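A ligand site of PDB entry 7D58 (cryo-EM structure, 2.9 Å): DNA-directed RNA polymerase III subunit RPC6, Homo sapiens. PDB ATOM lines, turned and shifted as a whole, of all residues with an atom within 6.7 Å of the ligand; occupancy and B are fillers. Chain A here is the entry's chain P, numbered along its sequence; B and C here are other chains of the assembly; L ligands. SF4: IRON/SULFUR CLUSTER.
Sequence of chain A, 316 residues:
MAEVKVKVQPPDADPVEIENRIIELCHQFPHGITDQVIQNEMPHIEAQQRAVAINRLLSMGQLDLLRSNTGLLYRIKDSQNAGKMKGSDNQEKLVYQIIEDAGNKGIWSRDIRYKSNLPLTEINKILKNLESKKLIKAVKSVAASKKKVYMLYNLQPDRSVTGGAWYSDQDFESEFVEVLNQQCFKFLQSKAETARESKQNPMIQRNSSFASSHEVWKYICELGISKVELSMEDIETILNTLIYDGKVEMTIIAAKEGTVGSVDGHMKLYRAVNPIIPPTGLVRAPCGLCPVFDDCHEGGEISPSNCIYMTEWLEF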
ATOM      1  N   ALA A 285       5.344 -40.576  27.583  1.00  0.00           N
ATOM      2  CA  ALA A 285       5.315 -39.340  26.826  1.00  0.00           C
ATOM      3  C   ALA A 285       5.877 -38.201  27.657  1.00  0.00           C
ATOM      4  O   ALA A 285       5.689 -38.164  28.878  1.00  0.00           O
ATOM      5  CB  ALA A 285       3.893 -39.014  26.380  1.00  0.00           C
ATOM      6  N   PRO A 286       6.591 -37.253  27.032  1.00  0.00           N
ATOM      7  CA  PRO A 286       7.181 -36.151  27.806  1.00  0.00           C
ATOM      8  C   PRO A 286       6.166 -35.200  28.409  1.00  0.00           C
ATOM      9  O   PRO A 286       6.545 -34.391  29.274  1.00  0.00           O
ATOM     10  CB  PRO A 286       8.076 -35.438  26.775  1.00  0.00           C
ATOM     11  CG  PRO A 286       7.479 -35.789  25.459  1.00  0.00           C
ATOM     12  CD  PRO A 286       6.915 -37.171  25.601  1.00  0.00           C
ATOM     13  N   CYS A 287       4.901 -35.255  27.983  1.00  0.00           N
ATOM     14  CA  CYS A 287       3.885 -34.394  28.571  1.00  0.00           C
ATOM     15  C   CYS A 287       3.583 -34.745  30.028  1.00  0.00           C
ATOM     16  O   CYS A 287       3.064 -33.900  30.752  1.00  0.00           O
ATOM     17  CB  CYS A 287       2.593 -34.473  27.750  1.00  0.00           C
ATOM     18  SG  CYS A 287       2.766 -33.908  26.037  1.00  0.00           S
ATOM     19  N   GLY A 288       3.883 -35.977  30.444  1.00  0.00           N
ATOM     20  CA  GLY A 288       3.667 -36.338  31.840  1.00  0.00           C
ATOM     21  C   GLY A 288       4.727 -35.773  32.762  1.00  0.00           C
ATOM     22  O   GLY A 288       4.444 -35.464  33.923  1.00  0.00           O
ATOM     23  N   LEU A 289       5.953 -35.642  32.268  1.00  0.00           N
ATOM     24  CA  LEU A 289       7.043 -35.067  33.040  1.00  0.00           C
ATOM     25  C   LEU A 289       7.066 -33.542  33.006  1.00  0.00           C
ATOM     26  O   LEU A 289       7.827 -32.936  33.759  1.00  0.00           O
ATOM     27  CB  LEU A 289       8.397 -35.589  32.537  1.00  0.00           C
ATOM     28  CG  LEU A 289       8.924 -36.953  33.002  1.00  0.00           C
ATOM     29  CD1 LEU A 289       9.056 -37.014  34.519  1.00  0.00           C
ATOM     30  CD2 LEU A 289       8.073 -38.085  32.467  1.00  0.00           C
ATOM     31  N   CYS A 290       6.260 -32.930  32.143  1.00  0.00           N
ATOM     32  CA  CYS A 290       6.300 -31.490  31.945  1.00  0.00           C
ATOM     33  C   CYS A 290       5.836 -30.757  33.200  1.00  0.00           C
ATOM     34  O   CYS A 290       4.704 -30.979  33.653  1.00  0.00           O
ATOM     35  CB  CYS A 290       5.432 -31.101  30.758  1.00  0.00           C
ATOM     36  SG  CYS A 290       5.666 -29.404  30.190  1.00  0.00           S
ATOM     37  N   PRO A 291       6.661 -29.899  33.795  1.00  0.00           N
ATOM     38  CA  PRO A 291       6.194 -29.128  34.955  1.00  0.00           C
ATOM     39  C   PRO A 291       5.249 -28.004  34.570  1.00  0.00           C
ATOM     40  O   PRO A 291       4.358 -27.663  35.373  1.00  0.00           O
ATOM     41  CB  PRO A 291       7.499 -28.584  35.554  1.00  0.00           C
ATOM     42  CG  PRO A 291       8.435 -28.489  34.397  1.00  0.00           C
ATOM     43  CD  PRO A 291       8.069 -29.606  33.454  1.00  0.00           C
ATOM     44  N   VAL A 292       5.392 -27.420  33.389  1.00  0.00           N
ATOM     45  CA  VAL A 292       4.481 -26.379  32.926  1.00  0.00           C
ATOM     46  C   VAL A 292       3.349 -27.018  32.127  1.00  0.00           C
ATOM     47  O   VAL A 292       3.436 -27.173  30.906  1.00  0.00           O
ATOM     48  CB  VAL A 292       5.237 -25.299  32.111  1.00  0.00           C
ATOM     49  CG1 VAL A 292       6.084 -24.460  33.050  1.00  0.00           C
ATOM     50  CG2 VAL A 292       6.135 -25.922  31.063  1.00  0.00           C
ATOM     51  N   PHE A 293       2.275 -27.383  32.817  1.00  0.00           N
ATOM     52  CA  PHE A 293       1.140 -28.055  32.195  1.00  0.00           C
ATOM     53  C   PHE A 293      -0.066 -27.146  32.026  1.00  0.00           C
ATOM     54  O   PHE A 293      -0.860 -27.352  31.093  1.00  0.00           O
ATOM     55  CB  PHE A 293       0.736 -29.275  33.034  1.00  0.00           C
ATOM     56  CG  PHE A 293      -0.393 -30.064  32.439  1.00  0.00           C
ATOM     57  CD1 PHE A 293      -0.194 -30.902  31.358  1.00  0.00           C
ATOM     58  CD2 PHE A 293      -1.673 -29.975  32.986  1.00  0.00           C
ATOM     59  CE1 PHE A 293      -1.236 -31.638  30.819  1.00  0.00           C
ATOM     60  CE2 PHE A 293      -2.719 -30.699  32.452  1.00  0.00           C
ATOM     61  CZ  PHE A 293      -2.499 -31.536  31.366  1.00  0.00           C
ATOM     62  N   ASP A 294      -0.225 -26.131  32.891  1.00  0.00           N
ATOM     63  CA  ASP A 294      -1.360 -25.230  32.778  1.00  0.00           C
ATOM     64  C   ASP A 294      -1.140 -24.212  31.669  1.00  0.00           C
ATOM     65  O   ASP A 294      -2.074 -23.856  30.934  1.00  0.00           O
ATOM     66  CB  ASP A 294      -1.594 -24.522  34.116  1.00  0.00           C
ATOM     67  CG  ASP A 294      -2.090 -25.454  35.191  1.00  0.00           C
ATOM     68  OD1 ASP A 294      -2.777 -26.439  34.862  1.00  0.00           O
ATOM     69  OD2 ASP A 294      -1.791 -25.205  36.378  1.00  0.00           O
ATOM     70  N   ASP A 295       0.095 -23.717  31.528  1.00  0.00           N
ATOM     71  CA  ASP A 295       0.380 -22.686  30.542  1.00  0.00           C
ATOM     72  C   ASP A 295       0.428 -23.256  29.134  1.00  0.00           C
ATOM     73  O   ASP A 295       0.361 -22.517  28.143  1.00  0.00           O
ATOM     74  CB  ASP A 295       1.697 -21.988  30.889  1.00  0.00           C
ATOM     75  CG  ASP A 295       1.809 -21.658  32.364  1.00  0.00           C
ATOM     76  OD1 ASP A 295       2.660 -22.272  33.046  1.00  0.00           O
ATOM     77  OD2 ASP A 295       1.043 -20.797  32.849  1.00  0.00           O
ATOM     78  N   CYS A 296       0.566 -24.585  29.015  1.00  0.00           N
ATOM     79  CA  CYS A 296       0.636 -25.242  27.711  1.00  0.00           C
ATOM     80  C   CYS A 296      -0.643 -25.025  26.911  1.00  0.00           C
ATOM     81  O   CYS A 296      -1.710 -25.532  27.270  1.00  0.00           O
ATOM     82  CB  CYS A 296       0.897 -26.731  27.883  1.00  0.00           C
ATOM     83  SG  CYS A 296       1.119 -27.636  26.330  1.00  0.00           S
ATOM     84  N   HIS A 297      -0.540 -24.274  25.811  1.00  0.00           N
ATOM     85  CA  HIS A 297      -1.680 -24.024  24.942  1.00  0.00           C
ATOM     86  C   HIS A 297      -1.163 -23.510  23.606  1.00  0.00           C
ATOM     87  O   HIS A 297      -0.201 -22.738  23.556  1.00  0.00           O
ATOM     88  CB  HIS A 297      -2.656 -23.013  25.548  1.00  0.00           C
ATOM     89  CG  HIS A 297      -2.096 -21.629  25.677  1.00  0.00           C
ATOM     90  ND1 HIS A 297      -1.246 -21.251  26.690  1.00  0.00           N
ATOM     91  CD2 HIS A 297      -2.276 -20.527  24.904  1.00  0.00           C
ATOM     92  CE1 HIS A 297      -0.914 -19.981  26.542  1.00  0.00           C
ATOM     93  NE2 HIS A 297      -1.530 -19.518  25.462  1.00  0.00           N
ATOM     94  N   ILE A 302       4.226 -20.868  25.347  1.00  0.00           N
ATOM     95  CA  ILE A 302       4.692 -22.253  25.395  1.00  0.00           C
ATOM     96  C   ILE A 302       3.593 -23.222  24.963  1.00  0.00           C
ATOM     97  O   ILE A 302       2.479 -23.204  25.501  1.00  0.00           O
ATOM     98  CB  ILE A 302       5.184 -22.604  26.814  1.00  0.00           C
ATOM     99  CG1 ILE A 302       6.202 -21.565  27.287  1.00  0.00           C
ATOM    100  CG2 ILE A 302       5.772 -24.005  26.833  1.00  0.00           C
ATOM    101  CD1 ILE A 302       6.373 -21.526  28.790  1.00  0.00           C
ATOM    102  N   SER A 303       3.924 -24.056  23.981  1.00  0.00           N
ATOM    103  CA  SER A 303       2.955 -24.871  23.265  1.00  0.00           C
ATOM    104  C   SER A 303       3.643 -26.128  22.746  1.00  0.00           C
ATOM    105  O   SER A 303       4.880 -26.194  22.748  1.00  0.00           O
ATOM    106  CB  SER A 303       2.329 -24.053  22.126  1.00  0.00           C
ATOM    107  OG  SER A 303       3.309 -23.715  21.159  1.00  0.00           O
ATOM    108  N   PRO A 304       2.895 -27.140  22.289  1.00  0.00           N
ATOM    109  CA  PRO A 304       3.543 -28.339  21.727  1.00  0.00           C
ATOM    110  C   PRO A 304       4.358 -28.088  20.467  1.00  0.00           C
ATOM    111  O   PRO A 304       5.120 -28.972  20.074  1.00  0.00           O
ATOM    112  CB  PRO A 304       2.361 -29.275  21.443  1.00  0.00           C
ATOM    113  CG  PRO A 304       1.166 -28.384  21.365  1.00  0.00           C
ATOM    114  CD  PRO A 304       1.432 -27.307  22.363  1.00  0.00           C
ATOM    115  N   SER A 305       4.219 -26.928  19.831  1.00  0.00           N
ATOM    116  CA  SER A 305       4.976 -26.667  18.613  1.00  0.00           C
ATOM    117  C   SER A 305       6.421 -26.283  18.927  1.00  0.00           C
ATOM    118  O   SER A 305       7.349 -26.829  18.329  1.00  0.00           O
ATOM    119  CB  SER A 305       4.294 -25.570  17.797  1.00  0.00           C
ATOM    120  OG  SER A 305       3.022 -25.982  17.345  1.00  0.00           O
ATOM    121  N   CYS A 307       8.021 -26.612  21.876  1.00  0.00           N
ATOM    122  CA  CYS A 307       8.388 -27.220  23.153  1.00  0.00           C
ATOM    123  C   CYS A 307       9.802 -27.804  23.066  1.00  0.00           C
ATOM    124  O   CYS A 307      10.134 -28.518  22.124  1.00  0.00           O
ATOM    125  CB  CYS A 307       7.391 -28.308  23.538  1.00  0.00           C
ATOM    126  SG  CYS A 307       7.758 -29.135  25.104  1.00  0.00           S
ATOM    127  N   ILE A 308      10.628 -27.492  24.068  1.00  0.00           N
ATOM    128  CA  ILE A 308      11.983 -28.013  24.103  1.00  0.00           C
ATOM    129  C   ILE A 308      11.976 -29.489  24.455  1.00  0.00           C
ATOM    130  O   ILE A 308      12.757 -30.286  23.915  1.00  0.00           O
ATOM    131  CB  ILE A 308      12.848 -27.194  25.074  1.00  0.00           C
ATOM    132  CG1 ILE A 308      13.055 -25.775  24.541  1.00  0.00           C
ATOM    133  CG2 ILE A 308      14.192 -27.870  25.314  1.00  0.00           C
ATOM    134  CD1 ILE A 308      13.930 -24.912  25.416  1.00  0.00           C
ATOM    135  N   TYR A 309      11.086 -29.890  25.370  1.00  0.00           N
ATOM    136  CA  TYR A 309      11.018 -31.298  25.780  1.00  0.00           C
ATOM    137  C   TYR A 309      10.604 -32.184  24.611  1.00  0.00           C
ATOM    138  O   TYR A 309      11.152 -33.285  24.432  1.00  0.00           O
ATOM    139  CB  TYR A 309      10.052 -31.450  26.955  1.00  0.00           C
ATOM    140  CG  TYR A 309      10.323 -30.509  28.096  1.00  0.00           C
ATOM    141  CD1 TYR A 309      11.384 -30.725  28.967  1.00  0.00           C
ATOM    142  CD2 TYR A 309       9.507 -29.406  28.316  1.00  0.00           C
ATOM    143  CE1 TYR A 309      11.625 -29.861  30.016  1.00  0.00           C
ATOM    144  CE2 TYR A 309       9.748 -28.542  29.365  1.00  0.00           C
ATOM    145  CZ  TYR A 309      10.803 -28.772  30.210  1.00  0.00           C
ATOM    146  OH  TYR A 309      11.041 -27.903  31.251  1.00  0.00           O
ATOM    147  N   MET A 310       9.625 -31.742  23.824  1.00  0.00           N
ATOM    148  CA  MET A 310       9.174 -32.516  22.669  1.00  0.00           C
ATOM    149  C   MET A 310      10.310 -32.723  21.676  1.00  0.00           C
ATOM    150  O   MET A 310      10.520 -33.838  21.169  1.00  0.00           O
ATOM    151  CB  MET A 310       7.994 -31.821  21.999  1.00  0.00           C
ATOM    152  CG  MET A 310       6.722 -31.803  22.838  1.00  0.00           C
ATOM    153  SD  MET A 310       6.095 -33.451  23.232  1.00  0.00           S
ATOM    154  CE  MET A 310       5.656 -34.048  21.600  1.00  0.00           C
ATOM    155  N   LYS B 441      -5.330 -34.144  27.424  1.00  0.00           N
ATOM    156  CA  LYS B 441      -4.576 -33.012  26.911  1.00  0.00           C
ATOM    157  C   LYS B 441      -3.193 -33.430  26.444  1.00  0.00           C
ATOM    158  O   LYS B 441      -2.636 -32.864  25.500  1.00  0.00           O
ATOM    159  CB  LYS B 441      -4.485 -31.909  27.969  1.00  0.00           C
ATOM    160  CG  LYS B 441      -4.227 -30.534  27.359  1.00  0.00           C
ATOM    161  CD  LYS B 441      -4.535 -29.401  28.326  1.00  0.00           C
ATOM    162  CE  LYS B 441      -3.329 -29.044  29.176  1.00  0.00           C
ATOM    163  NZ  LYS B 441      -3.579 -27.841  30.022  1.00  0.00           N
ATOM    164  N   SER B 442      -2.629 -34.470  27.081  1.00  0.00           N
ATOM    165  CA  SER B 442      -1.366 -35.020  26.614  1.00  0.00           C
ATOM    166  C   SER B 442      -1.502 -35.602  25.207  1.00  0.00           C
ATOM    167  O   SER B 442      -0.671 -35.366  24.328  1.00  0.00           O
ATOM    168  CB  SER B 442      -0.861 -36.091  27.590  1.00  0.00           C
ATOM    169  OG  SER B 442       0.346 -36.671  27.136  1.00  0.00           O
ATOM    170  N   ASN B 445      -1.860 -32.773  22.727  1.00  0.00           N
ATOM    171  CA  ASN B 445      -0.573 -32.161  22.430  1.00  0.00           C
ATOM    172  C   ASN B 445       0.255 -33.038  21.507  1.00  0.00           C
ATOM    173  O   ASN B 445       0.929 -32.536  20.593  1.00  0.00           O
ATOM    174  CB  ASN B 445       0.177 -31.870  23.725  1.00  0.00           C
ATOM    175  CG  ASN B 445      -0.463 -30.766  24.546  1.00  0.00           C
ATOM    176  OD1 ASN B 445      -1.234 -29.957  24.025  1.00  0.00           O
ATOM    177  ND2 ASN B 445      -0.170 -30.744  25.841  1.00  0.00           N
ATOM    178  N   LEU B 446       0.228 -34.350  21.733  1.00  0.00           N
ATOM    179  CA  LEU B 446       0.946 -35.268  20.845  1.00  0.00           C
ATOM    180  C   LEU B 446       0.408 -35.197  19.421  1.00  0.00           C
ATOM    181  O   LEU B 446       1.178 -35.187  18.452  1.00  0.00           O
ATOM    182  CB  LEU B 446       0.857 -36.698  21.385  1.00  0.00           C
ATOM    183  CG  LEU B 446       1.643 -37.015  22.659  1.00  0.00           C
ATOM    184  CD1 LEU B 446       1.483 -38.471  23.050  1.00  0.00           C
ATOM    185  CD2 LEU B 446       3.108 -36.654  22.476  1.00  0.00           C
ATOM    186  N   ARG B 449       1.509 -31.950  17.814  1.00  0.00           N
ATOM    187  CA  ARG B 449       2.907 -32.010  17.438  1.00  0.00           C
ATOM    188  C   ARG B 449       3.124 -32.892  16.211  1.00  0.00           C
ATOM    189  O   ARG B 449       3.972 -32.581  15.370  1.00  0.00           O
ATOM    190  CB  ARG B 449       3.751 -32.511  18.607  1.00  0.00           C
ATOM    191  CG  ARG B 449       5.237 -32.626  18.296  1.00  0.00           C
ATOM    192  CD  ARG B 449       5.850 -31.275  17.981  1.00  0.00           C
ATOM    193  NE  ARG B 449       7.280 -31.367  17.706  1.00  0.00           N
ATOM    194  CZ  ARG B 449       8.017 -30.366  17.232  1.00  0.00           C
ATOM    195  NH1 ARG B 449       7.449 -29.190  16.990  1.00  0.00           N
ATOM    196  NH2 ARG B 449       9.309 -30.545  17.003  1.00  0.00           N
ATOM    197  N   PHE C  38      11.222 -22.592  29.952  1.00  0.00           N
ATOM    198  CA  PHE C  38      11.364 -24.051  30.047  1.00  0.00           C
ATOM    199  C   PHE C  38      12.321 -24.393  31.173  1.00  0.00           C
ATOM    200  O   PHE C  38      13.533 -24.514  30.946  1.00  0.00           O
ATOM    201  CB  PHE C  38      11.844 -24.658  28.728  1.00  0.00           C
ATOM    202  CG  PHE C  38      10.840 -24.604  27.628  1.00  0.00           C
ATOM    203  CD1 PHE C  38       9.892 -25.616  27.483  1.00  0.00           C
ATOM    204  CD2 PHE C  38      10.837 -23.567  26.712  1.00  0.00           C
ATOM    205  CE1 PHE C  38       8.970 -25.573  26.466  1.00  0.00           C
ATOM    206  CE2 PHE C  38       9.905 -23.516  25.690  1.00  0.00           C
ATOM    207  CZ  PHE C  38       8.980 -24.523  25.564  1.00  0.00           C
HETATM  208 FE1  SF4 L   1       4.531 -30.059  28.198  1.00  0.00          FE
HETATM  209 FE2  SF4 L   1       3.388 -28.263  26.506  1.00  0.00          FE
HETATM  210 FE3  SF4 L   1       5.539 -29.815  25.773  1.00  0.00          FE
HETATM  211 FE4  SF4 L   1       3.073 -31.031  26.184  1.00  0.00          FE
HETATM  212  S1  SF4 L   1       3.582 -29.473  24.552  1.00  0.00           S
HETATM  213  S2  SF4 L   1       5.140 -31.810  26.843  1.00  0.00           S
HETATM  214  S3  SF4 L   1       2.259 -29.714  27.883  1.00  0.00           S
HETATM  215  S4  SF4 L   1       5.496 -28.157  27.359  1.00  0.00           S
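The side-chain amide nitrogen (ND2) of Asn 445 of chain B sits close to a sulfur (S3) of the ligand.
An iron atom (FE2) of the ligand is bound by the side-chain sulfur (SG) of Cys 296.
N of Cys 287 sits close to S2 of the ligand (3.6 Å).
A sulfur (S2) of the ligand sits close to the side-chain sulfur of Cys 287 (3.3 Å).
The side-chain sulfur (SG) of Cys 290 binds an iron atom (FE1) of the ligand (2.4 Å).
The side-chain sulfur (SG) of Cys 307 binds an iron atom (FE3) of the ligand (2.4 Å).
SG of Cys 296 lies close to ND2 of Asn 445 of chain B, at 3.4 Å.
The side-chain amide nitrogen of Asn 445 of chain B sits close to the backbone carbonyl oxygen of Lys 441 of chain B (3.3 Å).
The side-chain sulfur of Cys 290 sits close to the backbone carbonyl oxygen of Val 292 (3.2 Å).
The side-chain sulfur (SG) of Cys 307 sits close to the backbone NH (N) of Tyr 309, at 3.4 Å.
The backbone NH (N) of Met 310 lies close to the side-chain sulfur (SG) of Cys 307, at 3.5 Å.
The backbone nitrogen (N) of Pro 304 sits close to a sulfur (S1) of the ligand.
Residues that only touch the ligand: Met 310 (3.7 Å), Ser 303 (3.8 Å) and Pro 286 (3.8 Å).
Hydrophobic or aromatic side chains that line the ligand: Pro 304 and Met 310.
Of the 27 residues printed, 9 come within 4 Å of the ligand.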
